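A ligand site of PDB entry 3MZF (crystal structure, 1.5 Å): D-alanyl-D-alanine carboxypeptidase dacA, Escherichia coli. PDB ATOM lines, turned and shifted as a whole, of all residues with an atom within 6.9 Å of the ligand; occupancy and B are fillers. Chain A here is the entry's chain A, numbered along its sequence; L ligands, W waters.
Residues that only touch the ligand: Ala 43, Lys 47, Ser 86, Leu 153 and Arg 198.
Hydrophobic or aromatic side chains that line the ligand: Ala 43 and Leu 153.
12 residues have an atom within 4 Å of the ligand: Ala 43, Ser 44, Lys 47, Gly 85, Ser 86, Ser 87, Asn 112, Leu 153, Arg 198, Thr 214, Gly 215 and His 216.
The nearest printed residue that does not touch the ligand is Thr 217 (4.3 Å).
The side-chain hydroxyl of Ser 44 is in hydrogen-bond range of the side-chain amino group of Lys 47 (3.2 Å).
ND2 of Asn 112 lies within hydrogen-bond range of OG of Ser 86 (2.9 Å).
The side-chain amide oxygen (OD1) of Asn 112 lies within hydrogen-bond range of the side-chain amino group (NZ) of Lys 47 (2.8 Å).
N of Asn 223 lies within hydrogen-bond range of O of Gly 215 (2.8 Å).
The backbone carbonyl oxygen (O) of Ser 110 is in hydrogen-bond range of the side-chain hydroxyl (OG) of Ser 87 (2.6 Å).
The side-chain amino group of Lys 47 lies within hydrogen-bond range of the backbone carbonyl oxygen of His 151 (3.2 Å).
NZ of Lys 47 sits at hydrogen-bond distance from OG of Ser 110 (3.0 Å).
The guanidinium group (NE) of Arg 198 lies within hydrogen-bond range of the backbone carbonyl oxygen (O) of Gln 109, 2.8 Å away.
Water W3 bridges O4 of the ligand and NH1 of Arg 198.
Water W1 lies within hydrogen-bond range of O of Thr 214 (2.7 Å), OG of Ser 110 (2.8 Å), N1 of the ligand (2.8 Å) and OG of Ser 44 (3.5 Å).
Water W2 bridges the guanidinium group of Arg 198 (2.9 Å) and a nitrogen (N2) of the ligand (3.4 Å).
An oxygen (O1) of the ligand sits close to the backbone NH of Ser 44, 2.8 Å away.
A carbon (C1) of the ligand is bonded to the side-chain hydroxyl (OG) of Ser 44.
O3 of the ligand sits at hydrogen-bond distance from OG1 of Thr 214.
N of His 216 lies within hydrogen-bond range of O1 of the ligand (3.0 Å).
O2 of the ligand sits at hydrogen-bond distance from ND2 of Asn 112 (3.0 Å).
The backbone carbonyl oxygen (O) of Gly 85 lies within hydrogen-bond range of a nitrogen (N2) of the ligand, 3.1 Å away.
N of Gly 215 sits close to O3 of the ligand, at 3.2 Å.
N of Ser 87 sits at hydrogen-bond distance from O2 of the ligand (3.3 Å).
The side-chain hydroxyl (OG) of Ser 87 lies within hydrogen-bond range of an oxygen (O2) of the ligand (3.2 Å).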
ATOM      1  N   PRO A  42      35.254  -6.162 -13.521  1.00  0.00           N
ATOM      2  CA  PRO A  42      34.484  -7.379 -13.254  1.00  0.00           C
ATOM      3  C   PRO A  42      32.994  -7.211 -13.489  1.00  0.00           C
ATOM      4  O   PRO A  42      32.263  -8.213 -13.606  1.00  0.00           O
ATOM      5  CB  PRO A  42      34.746  -7.613 -11.752  1.00  0.00           C
ATOM      6  CG  PRO A  42      34.997  -6.265 -11.190  1.00  0.00           C
ATOM      7  CD  PRO A  42      35.622  -5.449 -12.289  1.00  0.00           C
ATOM      8  N   ALA A  43      32.529  -5.960 -13.528  1.00  0.00           N
ATOM      9  CA  ALA A  43      31.104  -5.653 -13.620  1.00  0.00           C
ATOM     10  C   ALA A  43      30.318  -6.498 -12.603  1.00  0.00           C
ATOM     11  O   ALA A  43      30.730  -6.582 -11.432  1.00  0.00           O
ATOM     12  CB  ALA A  43      30.590  -5.874 -15.059  1.00  0.00           C
ATOM     13  N   SER A  44      29.217  -7.112 -13.026  1.00  0.00           N
ATOM     14  CA  SER A  44      28.319  -7.834 -12.094  1.00  0.00           C
ATOM     15  C   SER A  44      28.938  -9.053 -11.441  1.00  0.00           C
ATOM     16  O   SER A  44      28.376  -9.573 -10.490  1.00  0.00           O
ATOM     17  CB  SER A  44      27.025  -8.258 -12.763  1.00  0.00           C
ATOM     18  OG  SER A  44      26.200  -7.142 -12.971  1.00  0.00           O
ATOM     19  N   LEU A  45      30.075  -9.518 -11.958  1.00  0.00           N
ATOM     20  CA  LEU A  45      30.767 -10.646 -11.306  1.00  0.00           C
ATOM     21  C   LEU A  45      31.163 -10.280  -9.865  1.00  0.00           C
ATOM     22  O   LEU A  45      31.366 -11.150  -9.034  1.00  0.00           O
ATOM     23  CB  LEU A  45      31.985 -11.096 -12.106  1.00  0.00           C
ATOM     24  CG  LEU A  45      31.737 -11.691 -13.499  1.00  0.00           C
ATOM     25  CD1 LEU A  45      33.023 -12.256 -14.055  1.00  0.00           C
ATOM     26  CD2 LEU A  45      30.677 -12.769 -13.451  1.00  0.00           C
ATOM     27  N   LYS A  47      29.308  -9.332  -7.720  1.00  0.00           N
ATOM     28  CA  LYS A  47      28.238  -9.866  -6.878  1.00  0.00           C
ATOM     29  C   LYS A  47      28.501 -11.285  -6.383  1.00  0.00           C
ATOM     30  O   LYS A  47      27.900 -11.715  -5.411  1.00  0.00           O
ATOM     31  CB  LYS A  47      26.901  -9.786  -7.605  1.00  0.00           C
ATOM     32  CG  LYS A  47      26.435  -8.394  -7.844  1.00  0.00           C
ATOM     33  CD  LYS A  47      24.981  -8.402  -8.260  1.00  0.00           C
ATOM     34  CE  LYS A  47      24.530  -7.010  -8.663  1.00  0.00           C
ATOM     35  NZ  LYS A  47      25.061  -6.570  -9.999  1.00  0.00           N
ATOM     36  N   PHE A  83      21.752   3.900 -10.266  1.00  0.00           N
ATOM     37  CA  PHE A  83      21.136   2.651 -10.716  1.00  0.00           C
ATOM     38  C   PHE A  83      20.598   2.687 -12.162  1.00  0.00           C
ATOM     39  O   PHE A  83      20.117   1.678 -12.675  1.00  0.00           O
ATOM     40  CB  PHE A  83      19.973   2.302  -9.801  1.00  0.00           C
ATOM     41  CG  PHE A  83      20.383   1.907  -8.382  1.00  0.00           C
ATOM     42  CD1 PHE A  83      19.641   2.361  -7.308  1.00  0.00           C
ATOM     43  CD2 PHE A  83      21.472   1.074  -8.154  1.00  0.00           C
ATOM     44  CE1 PHE A  83      19.983   1.994  -5.989  1.00  0.00           C
ATOM     45  CE2 PHE A  83      21.823   0.711  -6.835  1.00  0.00           C
ATOM     46  CZ  PHE A  83      21.070   1.184  -5.766  1.00  0.00           C
ATOM     47  N   GLY A  85      19.574   2.254 -15.730  1.00  0.00           N
ATOM     48  CA  GLY A  85      19.843   1.280 -16.791  1.00  0.00           C
ATOM     49  C   GLY A  85      20.439  -0.035 -16.311  1.00  0.00           C
ATOM     50  O   GLY A  85      20.866  -0.860 -17.122  1.00  0.00           O
ATOM     51  N   SER A  86      20.464  -0.217 -14.993  1.00  0.00           N
ATOM     52  CA  SER A  86      21.100  -1.394 -14.418  1.00  0.00           C
ATOM     53  C   SER A  86      20.059  -2.431 -13.985  1.00  0.00           C
ATOM     54  O   SER A  86      18.860  -2.169 -14.034  1.00  0.00           O
ATOM     55  CB  SER A  86      21.992  -0.970 -13.248  1.00  0.00           C
ATOM     56  OG  SER A  86      21.218  -0.691 -12.079  1.00  0.00           O
ATOM     57  N   SER A  87      20.529  -3.597 -13.588  1.00  0.00           N
ATOM     58  CA  SER A  87      19.630  -4.636 -13.124  1.00  0.00           C
ATOM     59  C   SER A  87      19.138  -4.323 -11.714  1.00  0.00           C
ATOM     60  O   SER A  87      19.931  -4.012 -10.825  1.00  0.00           O
ATOM     61  CB  SER A  87      20.320  -6.002 -13.172  1.00  0.00           C
ATOM     62  OG  SER A  87      21.667  -5.909 -12.757  1.00  0.00           O
ATOM     63  N   LEU A  88      17.823  -4.396 -11.527  1.00  0.00           N
ATOM     64  CA  LEU A  88      17.206  -3.961 -10.271  1.00  0.00           C
ATOM     65  C   LEU A  88      16.090  -4.886  -9.821  1.00  0.00           C
ATOM     66  O   LEU A  88      15.415  -5.512 -10.634  1.00  0.00           O
ATOM     67  CB  LEU A  88      16.686  -2.523 -10.368  1.00  0.00           C
ATOM     68  CG  LEU A  88      17.721  -1.422 -10.655  1.00  0.00           C
ATOM     69  CD1 LEU A  88      17.057  -0.126 -11.095  1.00  0.00           C
ATOM     70  CD2 LEU A  88      18.638  -1.158  -9.459  1.00  0.00           C
ATOM     71  N   GLN A 109      18.935 -12.316 -10.411  1.00  0.00           N
ATOM     72  CA  GLN A 109      18.581 -11.100 -11.142  1.00  0.00           C
ATOM     73  C   GLN A 109      19.734 -10.083 -11.201  1.00  0.00           C
ATOM     74  O   GLN A 109      19.706  -9.155 -12.007  1.00  0.00           O
ATOM     75  CB  GLN A 109      17.357 -10.471 -10.454  1.00  0.00           C
ATOM     76  CG  GLN A 109      16.632  -9.355 -11.189  1.00  0.00           C
ATOM     77  CD  GLN A 109      15.314  -8.960 -10.504  1.00  0.00           C
ATOM     78  OE1 GLN A 109      14.978  -9.460  -9.428  1.00  0.00           O
ATOM     79  NE2 GLN A 109      14.564  -8.072 -11.155  1.00  0.00           N
ATOM     80  N   SER A 110      20.770 -10.273 -10.376  1.00  0.00           N
ATOM     81  CA  SER A 110      21.868  -9.309 -10.298  1.00  0.00           C
ATOM     82  C   SER A 110      21.371  -7.923  -9.874  1.00  0.00           C
ATOM     83  O   SER A 110      21.851  -6.902 -10.369  1.00  0.00           O
ATOM     84  CB  SER A 110      22.615  -9.219 -11.639  1.00  0.00           C
ATOM     85  OG  SER A 110      23.982  -8.962 -11.445  1.00  0.00           O
ATOM     86  N   ASN A 112      21.081  -4.615  -8.211  1.00  0.00           N
ATOM     87  CA  ASN A 112      22.030  -3.722  -7.585  1.00  0.00           C
ATOM     88  C   ASN A 112      21.496  -3.109  -6.299  1.00  0.00           C
ATOM     89  O   ASN A 112      22.252  -2.909  -5.342  1.00  0.00           O
ATOM     90  CB  ASN A 112      22.473  -2.622  -8.549  1.00  0.00           C
ATOM     91  CG  ASN A 112      23.233  -3.177  -9.736  1.00  0.00           C
ATOM     92  OD1 ASN A 112      24.147  -3.975  -9.577  1.00  0.00           O
ATOM     93  ND2 ASN A 112      22.840  -2.770 -10.921  1.00  0.00           N
ATOM     94  N   HIS A 151      28.082  -3.904  -5.599  1.00  0.00           N
ATOM     95  CA  HIS A 151      27.338  -4.400  -6.748  1.00  0.00           C
ATOM     96  C   HIS A 151      28.110  -4.412  -8.068  1.00  0.00           C
ATOM     97  O   HIS A 151      27.726  -5.129  -9.001  1.00  0.00           O
ATOM     98  CB  HIS A 151      26.030  -3.606  -6.940  1.00  0.00           C
ATOM     99  CG  HIS A 151      26.136  -2.168  -6.583  1.00  0.00           C
ATOM    100  ND1 HIS A 151      27.190  -1.370  -7.014  1.00  0.00           N
ATOM    101  CD2 HIS A 151      25.357  -1.379  -5.817  1.00  0.00           C
ATOM    102  CE1 HIS A 151      27.033  -0.145  -6.532  1.00  0.00           C
ATOM    103  NE2 HIS A 151      25.925  -0.126  -5.796  1.00  0.00           N
ATOM    104  N   GLY A 152      29.190  -3.626  -8.124  1.00  0.00           N
ATOM    105  CA  GLY A 152      29.931  -3.400  -9.373  1.00  0.00           C
ATOM    106  C   GLY A 152      29.814  -1.980  -9.943  1.00  0.00           C
ATOM    107  O   GLY A 152      30.679  -1.546 -10.724  1.00  0.00           O
ATOM    108  N   LEU A 153      28.775  -1.239  -9.570  1.00  0.00           N
ATOM    109  CA  LEU A 153      28.579   0.118 -10.137  1.00  0.00           C
ATOM    110  C   LEU A 153      29.440   1.185  -9.467  1.00  0.00           C
ATOM    111  O   LEU A 153      29.803   1.066  -8.301  1.00  0.00           O
ATOM    112  CB  LEU A 153      27.125   0.558  -9.986  1.00  0.00           C
ATOM    113  CG  LEU A 153      25.973  -0.293 -10.473  1.00  0.00           C
ATOM    114  CD1 LEU A 153      24.724   0.295  -9.856  1.00  0.00           C
ATOM    115  CD2 LEU A 153      25.888  -0.284 -11.986  1.00  0.00           C
ATOM    116  N   ARG A 198      19.476 -14.964 -14.960  1.00  0.00           N
ATOM    117  CA  ARG A 198      20.179 -14.447 -16.142  1.00  0.00           C
ATOM    118  C   ARG A 198      21.174 -15.435 -16.779  1.00  0.00           C
ATOM    119  O   ARG A 198      21.634 -15.212 -17.899  1.00  0.00           O
ATOM    120  CB  ARG A 198      20.901 -13.133 -15.818  1.00  0.00           C
ATOM    121  CG  ARG A 198      19.972 -12.003 -15.421  1.00  0.00           C
ATOM    122  CD  ARG A 198      20.730 -10.718 -15.180  1.00  0.00           C
ATOM    123  NE  ARG A 198      19.831  -9.637 -14.774  1.00  0.00           N
ATOM    124  CZ  ARG A 198      19.110  -8.894 -15.604  1.00  0.00           C
ATOM    125  NH1 ARG A 198      19.194  -9.076 -16.919  1.00  0.00           N
ATOM    126  NH2 ARG A 198      18.316  -7.947 -15.134  1.00  0.00           N
ATOM    127  N   LYS A 213      27.473 -16.854 -12.378  1.00  0.00           N
ATOM    128  CA  LYS A 213      27.121 -15.448 -12.504  1.00  0.00           C
ATOM    129  C   LYS A 213      27.500 -14.889 -13.858  1.00  0.00           C
ATOM    130  O   LYS A 213      28.585 -15.165 -14.369  1.00  0.00           O
ATOM    131  CB  LYS A 213      27.861 -14.653 -11.425  1.00  0.00           C
ATOM    132  CG  LYS A 213      27.450 -13.200 -11.268  1.00  0.00           C
ATOM    133  CD  LYS A 213      26.602 -13.005 -10.012  1.00  0.00           C
ATOM    134  CE  LYS A 213      25.145 -12.824 -10.363  1.00  0.00           C
ATOM    135  NZ  LYS A 213      24.907 -11.474 -10.927  1.00  0.00           N
ATOM    136  N   THR A 214      26.601 -14.073 -14.394  1.00  0.00           N
ATOM    137  CA  THR A 214      26.831 -13.326 -15.620  1.00  0.00           C
ATOM    138  C   THR A 214      27.077 -11.852 -15.300  1.00  0.00           C
ATOM    139  O   THR A 214      26.705 -11.356 -14.232  1.00  0.00           O
ATOM    140  CB  THR A 214      25.594 -13.352 -16.516  1.00  0.00           C
ATOM    141  OG1 THR A 214      24.525 -12.672 -15.845  1.00  0.00           O
ATOM    142  CG2 THR A 214      25.185 -14.764 -16.827  1.00  0.00           C
ATOM    143  N   GLY A 215      27.669 -11.144 -16.238  1.00  0.00           N
ATOM    144  CA  GLY A 215      27.819  -9.700 -16.104  1.00  0.00           C
ATOM    145  C   GLY A 215      28.015  -9.044 -17.445  1.00  0.00           C
ATOM    146  O   GLY A 215      28.775  -9.527 -18.267  1.00  0.00           O
ATOM    147  N   HIS A 216      27.286  -7.959 -17.698  1.00  0.00           N
ATOM    148  CA  HIS A 216      27.578  -7.133 -18.855  1.00  0.00           C
ATOM    149  C   HIS A 216      27.446  -5.666 -18.534  1.00  0.00           C
ATOM    150  O   HIS A 216      26.447  -5.215 -17.964  1.00  0.00           O
ATOM    151  CB  HIS A 216      26.692  -7.451 -20.063  1.00  0.00           C
ATOM    152  CG  HIS A 216      26.933  -6.539 -21.225  1.00  0.00           C
ATOM    153  ND1 HIS A 216      26.136  -5.435 -21.493  1.00  0.00           N
ATOM    154  CD2 HIS A 216      27.918  -6.522 -22.155  1.00  0.00           C
ATOM    155  CE1 HIS A 216      26.604  -4.803 -22.552  1.00  0.00           C
ATOM    156  NE2 HIS A 216      27.684  -5.442 -22.974  1.00  0.00           N
ATOM    157  N   THR A 217      28.500  -4.941 -18.882  1.00  0.00           N
ATOM    158  CA  THR A 217      28.447  -3.497 -19.052  1.00  0.00           C
ATOM    159  C   THR A 217      29.145  -3.223 -20.380  1.00  0.00           C
ATOM    160  O   THR A 217      29.962  -4.028 -20.831  1.00  0.00           O
ATOM    161  CB  THR A 217      29.136  -2.746 -17.907  1.00  0.00           C
ATOM    162  OG1 THR A 217      30.506  -3.158 -17.809  1.00  0.00           O
ATOM    163  CG2 THR A 217      28.436  -2.996 -16.570  1.00  0.00           C
ATOM    164  N   ALA A 220      32.841  -3.490 -19.630  1.00  0.00           N
ATOM    165  CA  ALA A 220      33.436  -4.798 -19.313  1.00  0.00           C
ATOM    166  C   ALA A 220      33.239  -5.869 -20.391  1.00  0.00           C
ATOM    167  O   ALA A 220      33.876  -6.938 -20.357  1.00  0.00           O
ATOM    168  CB  ALA A 220      32.903  -5.313 -17.973  1.00  0.00           C
ATOM    169  N   GLY A 221      32.367  -5.595 -21.359  1.00  0.00           N
ATOM    170  CA  GLY A 221      31.966  -6.622 -22.327  1.00  0.00           C
ATOM    171  C   GLY A 221      31.102  -7.662 -21.639  1.00  0.00           C
ATOM    172  O   GLY A 221      30.480  -7.378 -20.625  1.00  0.00           O
ATOM    173  N   TYR A 222      31.072  -8.872 -22.205  1.00  0.00           N
ATOM    174  CA  TYR A 222      30.254  -9.945 -21.671  1.00  0.00           C
ATOM    175  C   TYR A 222      31.096 -10.873 -20.809  1.00  0.00           C
ATOM    176  O   TYR A 222      32.104 -11.411 -21.270  1.00  0.00           O
ATOM    177  CB  TYR A 222      29.605 -10.741 -22.793  1.00  0.00           C
ATOM    178  CG  TYR A 222      28.596  -9.957 -23.571  1.00  0.00           C
ATOM    179  CD1 TYR A 222      28.972  -9.210 -24.673  1.00  0.00           C
ATOM    180  CD2 TYR A 222      27.259  -9.955 -23.187  1.00  0.00           C
ATOM    181  CE1 TYR A 222      28.042  -8.476 -25.396  1.00  0.00           C
ATOM    182  CE2 TYR A 222      26.312  -9.231 -23.908  1.00  0.00           C
ATOM    183  CZ  TYR A 222      26.710  -8.504 -25.013  1.00  0.00           C
ATOM    184  OH  TYR A 222      25.800  -7.784 -25.731  1.00  0.00           O
ATOM    185  N   ASN A 223      30.651 -11.073 -19.583  1.00  0.00           N
ATOM    186  CA  ASN A 223      31.401 -11.830 -18.585  1.00  0.00           C
ATOM    187  C   ASN A 223      30.551 -12.969 -18.066  1.00  0.00           C
ATOM    188  O   ASN A 223      29.351 -12.821 -17.871  1.00  0.00           O
ATOM    189  CB  ASN A 223      31.696 -10.936 -17.374  1.00  0.00           C
ATOM    190  CG  ASN A 223      32.840  -9.958 -17.604  1.00  0.00           C
ATOM    191  OD1 ASN A 223      33.480  -9.957 -18.642  1.00  0.00           O
ATOM    192  ND2 ASN A 223      33.100  -9.122 -16.598  1.00  0.00           N
HETATM  193  C1  LIG L   1      26.306  -6.518 -14.179  1.00  0.00           C
HETATM  194  C2  LIG L   1      23.010  -6.870 -17.064  1.00  0.00           C
HETATM  195  C3  LIG L   1      25.215  -5.557 -14.558  1.00  0.00           C
HETATM  196  C4  LIG L   1      23.989  -6.392 -14.968  1.00  0.00           C
HETATM  197  C5  LIG L   1      23.764  -7.914 -16.740  1.00  0.00           C
HETATM  198  O1  LIG L   1      27.249  -6.771 -14.920  1.00  0.00           O
HETATM  199  C6  LIG L   1      24.896  -4.683 -13.334  1.00  0.00           C
HETATM  200  O2  LIG L   1      23.865  -3.736 -13.626  1.00  0.00           O
HETATM  201  C7  LIG L   1      26.125  -3.922 -12.814  1.00  0.00           C
HETATM  202  N1  LIG L   1      24.442  -7.625 -15.630  1.00  0.00           N
HETATM  203  C8  LIG L   1      23.914  -9.224 -17.410  1.00  0.00           C
HETATM  204  O3  LIG L   1      24.782 -10.017 -16.970  1.00  0.00           O
HETATM  205  O4  LIG L   1      23.189  -9.520 -18.388  1.00  0.00           O
HETATM  206  S1  LIG L   1      21.994  -6.778 -18.385  1.00  0.00           S
HETATM  207  C9  LIG L   1      21.218  -5.196 -18.454  1.00  0.00           C
HETATM  208  C10 LIG L   1      20.158  -5.090 -17.370  1.00  0.00           C
HETATM  209  N2  LIG L   1      19.700  -3.713 -17.411  1.00  0.00           N
HETATM  210  C11 LIG L   1      23.166  -5.739 -16.086  1.00  0.00           C
HETATM  211  O   HOH W   1      24.396  -9.925 -14.023  1.00  0.00           O
HETATM  212  O   HOH W   2      17.069  -5.614 -16.246  1.00  0.00           O
HETATM  213  O   HOH W   3      20.694 -10.567 -19.041  1.00  0.00           O
HETATM  214  O   HOH W   4      24.656  -1.987 -15.525  1.00  0.00           O
